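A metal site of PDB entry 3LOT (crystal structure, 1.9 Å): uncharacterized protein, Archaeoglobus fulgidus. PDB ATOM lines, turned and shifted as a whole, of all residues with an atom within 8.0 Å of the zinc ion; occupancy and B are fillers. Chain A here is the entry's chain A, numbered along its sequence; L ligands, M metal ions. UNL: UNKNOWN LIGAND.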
ATOM      1  N   ALA A  13       5.534  -6.575  35.648  1.00  0.00           N
ATOM      2  CA  ALA A  13       6.513  -7.274  34.819  1.00  0.00           C
ATOM      3  C   ALA A  13       7.810  -6.516  34.976  1.00  0.00           C
ATOM      4  O   ALA A  13       7.965  -5.409  34.466  1.00  0.00           O
ATOM      5  CB  ALA A  13       6.036  -7.311  33.351  1.00  0.00           C
ATOM      6  N   ILE A  14       8.735  -7.140  35.695  1.00  0.00           N
ATOM      7  CA  ILE A  14       9.845  -6.433  36.300  1.00  0.00           C
ATOM      8  C   ILE A  14      10.909  -5.927  35.295  1.00  0.00           C
ATOM      9  O   ILE A  14      11.507  -4.896  35.547  1.00  0.00           O
ATOM     10  CB  ILE A  14      10.525  -7.309  37.366  1.00  0.00           C
ATOM     11  CG1 ILE A  14       9.546  -7.695  38.490  1.00  0.00           C
ATOM     12  CG2 ILE A  14      11.799  -6.602  37.954  1.00  0.00           C
ATOM     13  CD1 ILE A  14       8.778  -6.548  39.121  1.00  0.00           C
ATOM     14  N   THR A  15      11.224  -6.664  34.231  1.00  0.00           N
ATOM     15  CA  THR A  15      12.375  -6.314  33.418  1.00  0.00           C
ATOM     16  C   THR A  15      12.290  -6.713  31.951  1.00  0.00           C
ATOM     17  O   THR A  15      12.620  -5.939  31.033  1.00  0.00           O
ATOM     18  CB  THR A  15      13.737  -6.817  34.069  1.00  0.00           C
ATOM     19  OG1 THR A  15      14.830  -6.275  33.332  1.00  0.00           O
ATOM     20  CG2 THR A  15      13.856  -8.333  34.077  1.00  0.00           C
ATOM     21  N   GLY A  16      11.828  -7.925  31.728  1.00  0.00           N
ATOM     22  CA  GLY A  16      11.554  -8.412  30.394  1.00  0.00           C
ATOM     23  C   GLY A  16      12.810  -8.744  29.598  1.00  0.00           C
ATOM     24  O   GLY A  16      13.882  -8.989  30.144  1.00  0.00           O
ATOM     25  N   ALA A  17      12.655  -8.712  28.279  1.00  0.00           N
ATOM     26  CA  ALA A  17      13.737  -8.989  27.320  1.00  0.00           C
ATOM     27  C   ALA A  17      13.773  -7.947  26.185  1.00  0.00           C
ATOM     28  O   ALA A  17      14.664  -7.983  25.365  1.00  0.00           O
ATOM     29  CB  ALA A  17      13.538 -10.386  26.708  1.00  0.00           C
ATOM     30  N   ILE A  18      12.815  -7.019  26.157  1.00  0.00           N
ATOM     31  CA  ILE A  18      12.697  -6.030  25.086  1.00  0.00           C
ATOM     32  C   ILE A  18      13.612  -4.818  25.334  1.00  0.00           C
ATOM     33  O   ILE A  18      14.472  -4.500  24.484  1.00  0.00           O
ATOM     34  CB  ILE A  18      11.252  -5.577  24.876  1.00  0.00           C
ATOM     35  CG1 ILE A  18      10.459  -6.634  24.104  1.00  0.00           C
ATOM     36  CG2 ILE A  18      11.194  -4.254  24.060  1.00  0.00           C
ATOM     37  CD1 ILE A  18      11.092  -8.073  24.038  1.00  0.00           C
ATOM     38  N   HIS A  50       5.976 -10.734  37.275  1.00  0.00           N
ATOM     39  CA  HIS A  50       6.401 -11.459  36.091  1.00  0.00           C
ATOM     40  C   HIS A  50       7.902 -11.279  35.887  1.00  0.00           C
ATOM     41  O   HIS A  50       8.405 -10.124  35.837  1.00  0.00           O
ATOM     42  CB  HIS A  50       5.624 -11.011  34.857  1.00  0.00           C
ATOM     43  CG  HIS A  50       6.147 -11.609  33.603  1.00  0.00           C
ATOM     44  ND1 HIS A  50       6.092 -12.974  33.350  1.00  0.00           N
ATOM     45  CD2 HIS A  50       6.826 -11.057  32.569  1.00  0.00           C
ATOM     46  CE1 HIS A  50       6.679 -13.217  32.195  1.00  0.00           C
ATOM     47  NE2 HIS A  50       7.147 -12.076  31.724  1.00  0.00           N
ATOM     48  N   ILE A  51       8.600 -12.420  35.782  1.00  0.00           N
ATOM     49  CA  ILE A  51      10.052 -12.510  35.846  1.00  0.00           C
ATOM     50  C   ILE A  51      10.675 -13.093  34.570  1.00  0.00           C
ATOM     51  O   ILE A  51      10.297 -14.186  34.108  1.00  0.00           O
ATOM     52  CB  ILE A  51      10.451 -13.471  37.055  1.00  0.00           C
ATOM     53  CG1 ILE A  51       9.913 -12.904  38.403  1.00  0.00           C
ATOM     54  CG2 ILE A  51      11.964 -13.657  37.146  1.00  0.00           C
ATOM     55  CD1 ILE A  51      10.498 -11.592  38.835  1.00  0.00           C
ATOM     56  N   HIS A  52      11.600 -12.307  33.974  1.00  0.00           N
ATOM     57  CA  HIS A  52      12.609 -12.797  33.000  1.00  0.00           C
ATOM     58  C   HIS A  52      13.968 -12.782  33.679  1.00  0.00           C
ATOM     59  O   HIS A  52      14.159 -12.023  34.628  1.00  0.00           O
ATOM     60  CB  HIS A  52      12.764 -11.855  31.811  1.00  0.00           C
ATOM     61  CG  HIS A  52      11.657 -11.884  30.837  1.00  0.00           C
ATOM     62  ND1 HIS A  52      11.858 -12.046  29.480  1.00  0.00           N
ATOM     63  CD2 HIS A  52      10.321 -11.729  31.004  1.00  0.00           C
ATOM     64  CE1 HIS A  52      10.693 -12.022  28.861  1.00  0.00           C
ATOM     65  NE2 HIS A  52       9.752 -11.843  29.768  1.00  0.00           N
ATOM     66  N   ASN A  84       5.288 -15.353  38.499  1.00  0.00           N
ATOM     67  CA  ASN A  84       5.040 -15.798  37.132  1.00  0.00           C
ATOM     68  C   ASN A  84       6.353 -15.803  36.358  1.00  0.00           C
ATOM     69  O   ASN A  84       6.984 -14.738  36.185  1.00  0.00           O
ATOM     70  CB  ASN A  84       3.985 -14.845  36.543  1.00  0.00           C
ATOM     71  CG  ASN A  84       3.648 -15.081  35.090  1.00  0.00           C
ATOM     72  OD1 ASN A  84       4.514 -15.313  34.263  1.00  0.00           O
ATOM     73  ND2 ASN A  84       2.371 -14.955  34.771  1.00  0.00           N
ATOM     74  N   VAL A  85       6.759 -16.996  35.869  1.00  0.00           N
ATOM     75  CA  VAL A  85       8.025 -17.170  35.141  1.00  0.00           C
ATOM     76  C   VAL A  85       7.820 -17.256  33.617  1.00  0.00           C
ATOM     77  O   VAL A  85       6.958 -17.982  33.128  1.00  0.00           O
ATOM     78  CB  VAL A  85       8.825 -18.406  35.704  1.00  0.00           C
ATOM     79  CG1 VAL A  85       9.766 -18.989  34.686  1.00  0.00           C
ATOM     80  CG2 VAL A  85       9.615 -17.983  36.954  1.00  0.00           C
ATOM     81  N   THR A  86       8.605 -16.482  32.856  1.00  0.00           N
ATOM     82  CA  THR A  86       8.469 -16.461  31.404  1.00  0.00           C
ATOM     83  C   THR A  86       8.912 -17.748  30.770  1.00  0.00           C
ATOM     84  O   THR A  86       9.870 -18.356  31.229  1.00  0.00           O
ATOM     85  CB  THR A  86       9.279 -15.309  30.745  1.00  0.00           C
ATOM     86  OG1 THR A  86       8.888 -15.158  29.373  1.00  0.00           O
ATOM     87  CG2 THR A  86      10.759 -15.567  30.827  1.00  0.00           C
ATOM     88  N   THR A  87       8.198 -18.178  29.722  1.00  0.00           N
ATOM     89  CA  THR A  87       8.721 -19.138  28.730  1.00  0.00           C
ATOM     90  C   THR A  87       8.816 -18.465  27.324  1.00  0.00           C
ATOM     91  O   THR A  87       9.070 -19.144  26.314  1.00  0.00           O
ATOM     92  CB  THR A  87       7.961 -20.461  28.670  1.00  0.00           C
ATOM     93  OG1 THR A  87       6.692 -20.320  27.981  1.00  0.00           O
ATOM     94  CG2 THR A  87       7.753 -21.102  30.104  1.00  0.00           C
ATOM     95  N   GLY A  88       8.638 -17.142  27.272  1.00  0.00           N
ATOM     96  CA  GLY A  88       8.786 -16.371  26.057  1.00  0.00           C
ATOM     97  C   GLY A  88      10.176 -15.744  25.901  1.00  0.00           C
ATOM     98  O   GLY A  88      10.663 -15.569  24.805  1.00  0.00           O
ATOM     99  N   GLY A  89      10.798 -15.423  27.031  1.00  0.00           N
ATOM    100  CA  GLY A  89      12.097 -14.831  27.060  1.00  0.00           C
ATOM    101  C   GLY A  89      13.144 -15.629  26.315  1.00  0.00           C
ATOM    102  O   GLY A  89      13.368 -16.807  26.583  1.00  0.00           O
ATOM    103  N   THR A 113       4.242 -18.013  31.614  1.00  0.00           N
ATOM    104  CA  THR A 113       3.755 -17.534  30.346  1.00  0.00           C
ATOM    105  C   THR A 113       3.745 -18.684  29.316  1.00  0.00           C
ATOM    106  O   THR A 113       4.568 -19.615  29.351  1.00  0.00           O
ATOM    107  CB  THR A 113       4.489 -16.271  29.803  1.00  0.00           C
ATOM    108  OG1 THR A 113       5.835 -16.561  29.392  1.00  0.00           O
ATOM    109  CG2 THR A 113       4.435 -15.119  30.797  1.00  0.00           C
ATOM    110  N   ASN A 115       3.015 -18.623  25.207  1.00  0.00           N
ATOM    111  CA  ASN A 115       2.738 -17.748  24.080  1.00  0.00           C
ATOM    112  C   ASN A 115       2.032 -18.510  22.951  1.00  0.00           C
ATOM    113  O   ASN A 115       2.428 -19.630  22.631  1.00  0.00           O
ATOM    114  CB  ASN A 115       4.030 -17.120  23.626  1.00  0.00           C
ATOM    115  CG  ASN A 115       4.566 -16.123  24.638  1.00  0.00           C
ATOM    116  OD1 ASN A 115       4.196 -14.958  24.602  1.00  0.00           O
ATOM    117  ND2 ASN A 115       5.444 -16.579  25.538  1.00  0.00           N
ATOM    118  N   PHE A 121       8.091 -10.083  15.808  1.00  0.00           N
ATOM    119  CA  PHE A 121       8.184  -9.402  17.100  1.00  0.00           C
ATOM    120  C   PHE A 121       9.396  -8.498  16.976  1.00  0.00           C
ATOM    121  O   PHE A 121      10.506  -8.913  17.249  1.00  0.00           O
ATOM    122  CB  PHE A 121       8.376 -10.460  18.226  1.00  0.00           C
ATOM    123  CG  PHE A 121       8.088  -9.951  19.613  1.00  0.00           C
ATOM    124  CD1 PHE A 121       8.712  -8.807  20.131  1.00  0.00           C
ATOM    125  CD2 PHE A 121       7.221 -10.646  20.449  1.00  0.00           C
ATOM    126  CE1 PHE A 121       8.415  -8.346  21.380  1.00  0.00           C
ATOM    127  CE2 PHE A 121       6.943 -10.173  21.720  1.00  0.00           C
ATOM    128  CZ  PHE A 121       7.528  -9.035  22.184  1.00  0.00           C
ATOM    129  N   GLU A 172      -0.469 -19.078  31.592  1.00  0.00           N
ATOM    130  CA  GLU A 172      -0.993 -17.734  31.283  1.00  0.00           C
ATOM    131  C   GLU A 172      -0.810 -17.546  29.774  1.00  0.00           C
ATOM    132  O   GLU A 172       0.317 -17.380  29.245  1.00  0.00           O
ATOM    133  CB  GLU A 172      -0.227 -16.639  32.022  1.00  0.00           C
ATOM    134  CG  GLU A 172      -0.750 -15.254  31.703  1.00  0.00           C
ATOM    135  CD  GLU A 172       0.052 -14.128  32.412  1.00  0.00           C
ATOM    136  OE1 GLU A 172       1.096 -13.713  31.893  1.00  0.00           O
ATOM    137  OE2 GLU A 172      -0.395 -13.643  33.456  1.00  0.00           O
ATOM    138  N   GLU A 174      -0.629 -16.063  26.438  1.00  0.00           N
ATOM    139  CA  GLU A 174      -0.354 -14.729  25.857  1.00  0.00           C
ATOM    140  C   GLU A 174      -0.834 -14.648  24.401  1.00  0.00           C
ATOM    141  O   GLU A 174      -0.375 -15.386  23.521  1.00  0.00           O
ATOM    142  CB  GLU A 174       1.124 -14.362  25.934  1.00  0.00           C
ATOM    143  CG  GLU A 174       1.898 -14.824  27.165  1.00  0.00           C
ATOM    144  CD  GLU A 174       1.482 -14.216  28.515  1.00  0.00           C
ATOM    145  OE1 GLU A 174       0.782 -13.230  28.511  1.00  0.00           O
ATOM    146  OE2 GLU A 174       1.824 -14.784  29.599  1.00  0.00           O
ATOM    147  N   TYR A 176      -1.398 -12.021  21.222  1.00  0.00           N
ATOM    148  CA  TYR A 176      -0.921 -10.744  20.664  1.00  0.00           C
ATOM    149  C   TYR A 176      -1.739 -10.367  19.424  1.00  0.00           C
ATOM    150  O   TYR A 176      -1.453  -9.383  18.748  1.00  0.00           O
ATOM    151  CB  TYR A 176       0.552 -10.826  20.274  1.00  0.00           C
ATOM    152  CG  TYR A 176       1.576 -11.163  21.353  1.00  0.00           C
ATOM    153  CD1 TYR A 176       1.705 -12.463  21.830  1.00  0.00           C
ATOM    154  CD2 TYR A 176       2.468 -10.235  21.795  1.00  0.00           C
ATOM    155  CE1 TYR A 176       2.661 -12.779  22.756  1.00  0.00           C
ATOM    156  CE2 TYR A 176       3.428 -10.531  22.759  1.00  0.00           C
ATOM    157  CZ  TYR A 176       3.515 -11.814  23.231  1.00  0.00           C
ATOM    158  OH  TYR A 176       4.447 -12.172  24.165  1.00  0.00           O
ATOM    159  N   GLN A 200      -4.025 -13.461  28.506  1.00  0.00           N
ATOM    160  CA  GLN A 200      -3.531 -12.117  28.587  1.00  0.00           C
ATOM    161  C   GLN A 200      -3.389 -11.535  27.198  1.00  0.00           C
ATOM    162  O   GLN A 200      -2.688 -12.068  26.367  1.00  0.00           O
ATOM    163  CB  GLN A 200      -2.196 -12.065  29.340  1.00  0.00           C
ATOM    164  CG  GLN A 200      -1.730 -10.664  29.605  1.00  0.00           C
ATOM    165  CD  GLN A 200      -0.740 -10.558  30.740  1.00  0.00           C
ATOM    166  OE1 GLN A 200      -0.988  -9.885  31.739  1.00  0.00           O
ATOM    167  NE2 GLN A 200       0.392 -11.240  30.595  1.00  0.00           N
ATOM    168  N   ILE A 202      -1.982  -8.773  24.743  1.00  0.00           N
ATOM    169  CA  ILE A 202      -0.795  -7.903  24.622  1.00  0.00           C
ATOM    170  C   ILE A 202      -0.920  -7.012  23.403  1.00  0.00           C
ATOM    171  O   ILE A 202      -1.033  -7.510  22.274  1.00  0.00           O
ATOM    172  CB  ILE A 202       0.495  -8.728  24.622  1.00  0.00           C
ATOM    173  CG1 ILE A 202       0.485  -9.594  25.905  1.00  0.00           C
ATOM    174  CG2 ILE A 202       1.734  -7.802  24.607  1.00  0.00           C
ATOM    175  CD1 ILE A 202       1.683 -10.381  26.256  1.00  0.00           C
ATOM    176  N   VAL A 237      -1.952  -6.197  28.699  1.00  0.00           N
ATOM    177  CA  VAL A 237      -0.721  -5.433  28.652  1.00  0.00           C
ATOM    178  C   VAL A 237      -0.844  -4.380  27.574  1.00  0.00           C
ATOM    179  O   VAL A 237      -1.040  -4.727  26.398  1.00  0.00           O
ATOM    180  CB  VAL A 237       0.512  -6.303  28.303  1.00  0.00           C
ATOM    181  CG1 VAL A 237       1.782  -5.375  28.156  1.00  0.00           C
ATOM    182  CG2 VAL A 237       0.752  -7.330  29.310  1.00  0.00           C
ATOM    183  N   ARG A 258      -1.632  -5.620  33.841  1.00  0.00           N
ATOM    184  CA  ARG A 258      -0.190  -5.700  34.035  1.00  0.00           C
ATOM    185  C   ARG A 258       0.516  -4.344  33.788  1.00  0.00           C
ATOM    186  O   ARG A 258       0.258  -3.671  32.794  1.00  0.00           O
ATOM    187  CB  ARG A 258       0.383  -6.754  33.097  1.00  0.00           C
ATOM    188  CG  ARG A 258       1.859  -6.874  33.120  1.00  0.00           C
ATOM    189  CD  ARG A 258       2.382  -8.131  32.427  1.00  0.00           C
ATOM    190  NE  ARG A 258       3.342  -7.772  31.385  1.00  0.00           N
ATOM    191  CZ  ARG A 258       4.008  -8.654  30.667  1.00  0.00           C
ATOM    192  NH1 ARG A 258       3.883  -9.956  30.921  1.00  0.00           N
ATOM    193  NH2 ARG A 258       4.808  -8.252  29.700  1.00  0.00           N
ATOM    194  N   GLU A 262       9.281  -3.752  32.232  1.00  0.00           N
ATOM    195  CA  GLU A 262       9.336  -4.604  31.032  1.00  0.00           C
ATOM    196  C   GLU A 262       8.582  -4.025  29.852  1.00  0.00           C
ATOM    197  O   GLU A 262       9.021  -4.161  28.724  1.00  0.00           O
ATOM    198  CB  GLU A 262       8.782  -5.992  31.333  1.00  0.00           C
ATOM    199  CG  GLU A 262       8.472  -6.790  30.164  1.00  0.00           C
ATOM    200  CD  GLU A 262       8.299  -8.286  30.503  1.00  0.00           C
ATOM    201  OE1 GLU A 262       8.565  -8.723  31.632  1.00  0.00           O
ATOM    202  OE2 GLU A 262       7.878  -9.014  29.615  1.00  0.00           O
ATOM    203  N   ASP A 263       7.443  -3.384  30.118  1.00  0.00           N
ATOM    204  CA  ASP A 263       6.530  -2.941  29.083  1.00  0.00           C
ATOM    205  C   ASP A 263       6.650  -1.414  28.832  1.00  0.00           C
ATOM    206  O   ASP A 263       6.400  -0.946  27.740  1.00  0.00           O
ATOM    207  CB  ASP A 263       5.052  -3.263  29.472  1.00  0.00           C
ATOM    208  CG  ASP A 263       4.805  -4.757  29.779  1.00  0.00           C
ATOM    209  OD1 ASP A 263       5.350  -5.596  29.002  1.00  0.00           O
ATOM    210  OD2 ASP A 263       4.006  -5.086  30.755  1.00  0.00           O
HETATM  211  O1  UNL L   1       6.306 -14.964  27.604  1.00  0.00           O
HETATM  212  O2  UNL L   1       6.151 -13.558  27.848  1.00  0.00           O
HETATM  213  O3  UNL L   1       7.139 -13.533  28.846  1.00  0.00           O
HETATM  214  O4  UNL L   1       5.597 -12.145  27.167  1.00  0.00           O
HETATM  215  O5  UNL L   1       5.550 -10.835  28.674  1.00  0.00           O
HETATM  216 ZN    ZN M   1       7.559 -11.296  29.635  1.00  0.00          ZN
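The backbone carbonyl oxygen (O) of His 50 sits at hydrogen-bond distance from the backbone NH (N) of Ile 14.
OE2 of Glu 262 sits close to NH2 of Arg 258 (3.2 Å).
N of Glu 262 lies within hydrogen-bond range of O of Ala 13, 3.1 Å away.
The side-chain hydroxyl (OG1) of Thr 86 sits close to a ring nitrogen (NE2) of His 52 (3.4 Å).
OE1 of Glu 262 sits close to N of Gly 16 (3.4 Å).
A ring nitrogen (ND1) of His 50 lies within hydrogen-bond range of the side-chain amide oxygen (OD1) of Asn 84, at 3.0 Å.
Of the 27 residues printed, 3 come within 4 Å of the zinc ion.
The nearest printed residue that does not touch the zinc ion is Thr 86 (4.1 Å).
The zinc ion is bound by a ring nitrogen (NE2) of His 52 (2.3 Å), a ring nitrogen (NE2) of His 50 (2.3 Å), an oxygen (O5) of the ligand (2.3 Å), the side-chain carboxylate (OE2) of Glu 262 (2.3 Å) and an oxygen (O3) of the ligand (2.4 Å).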
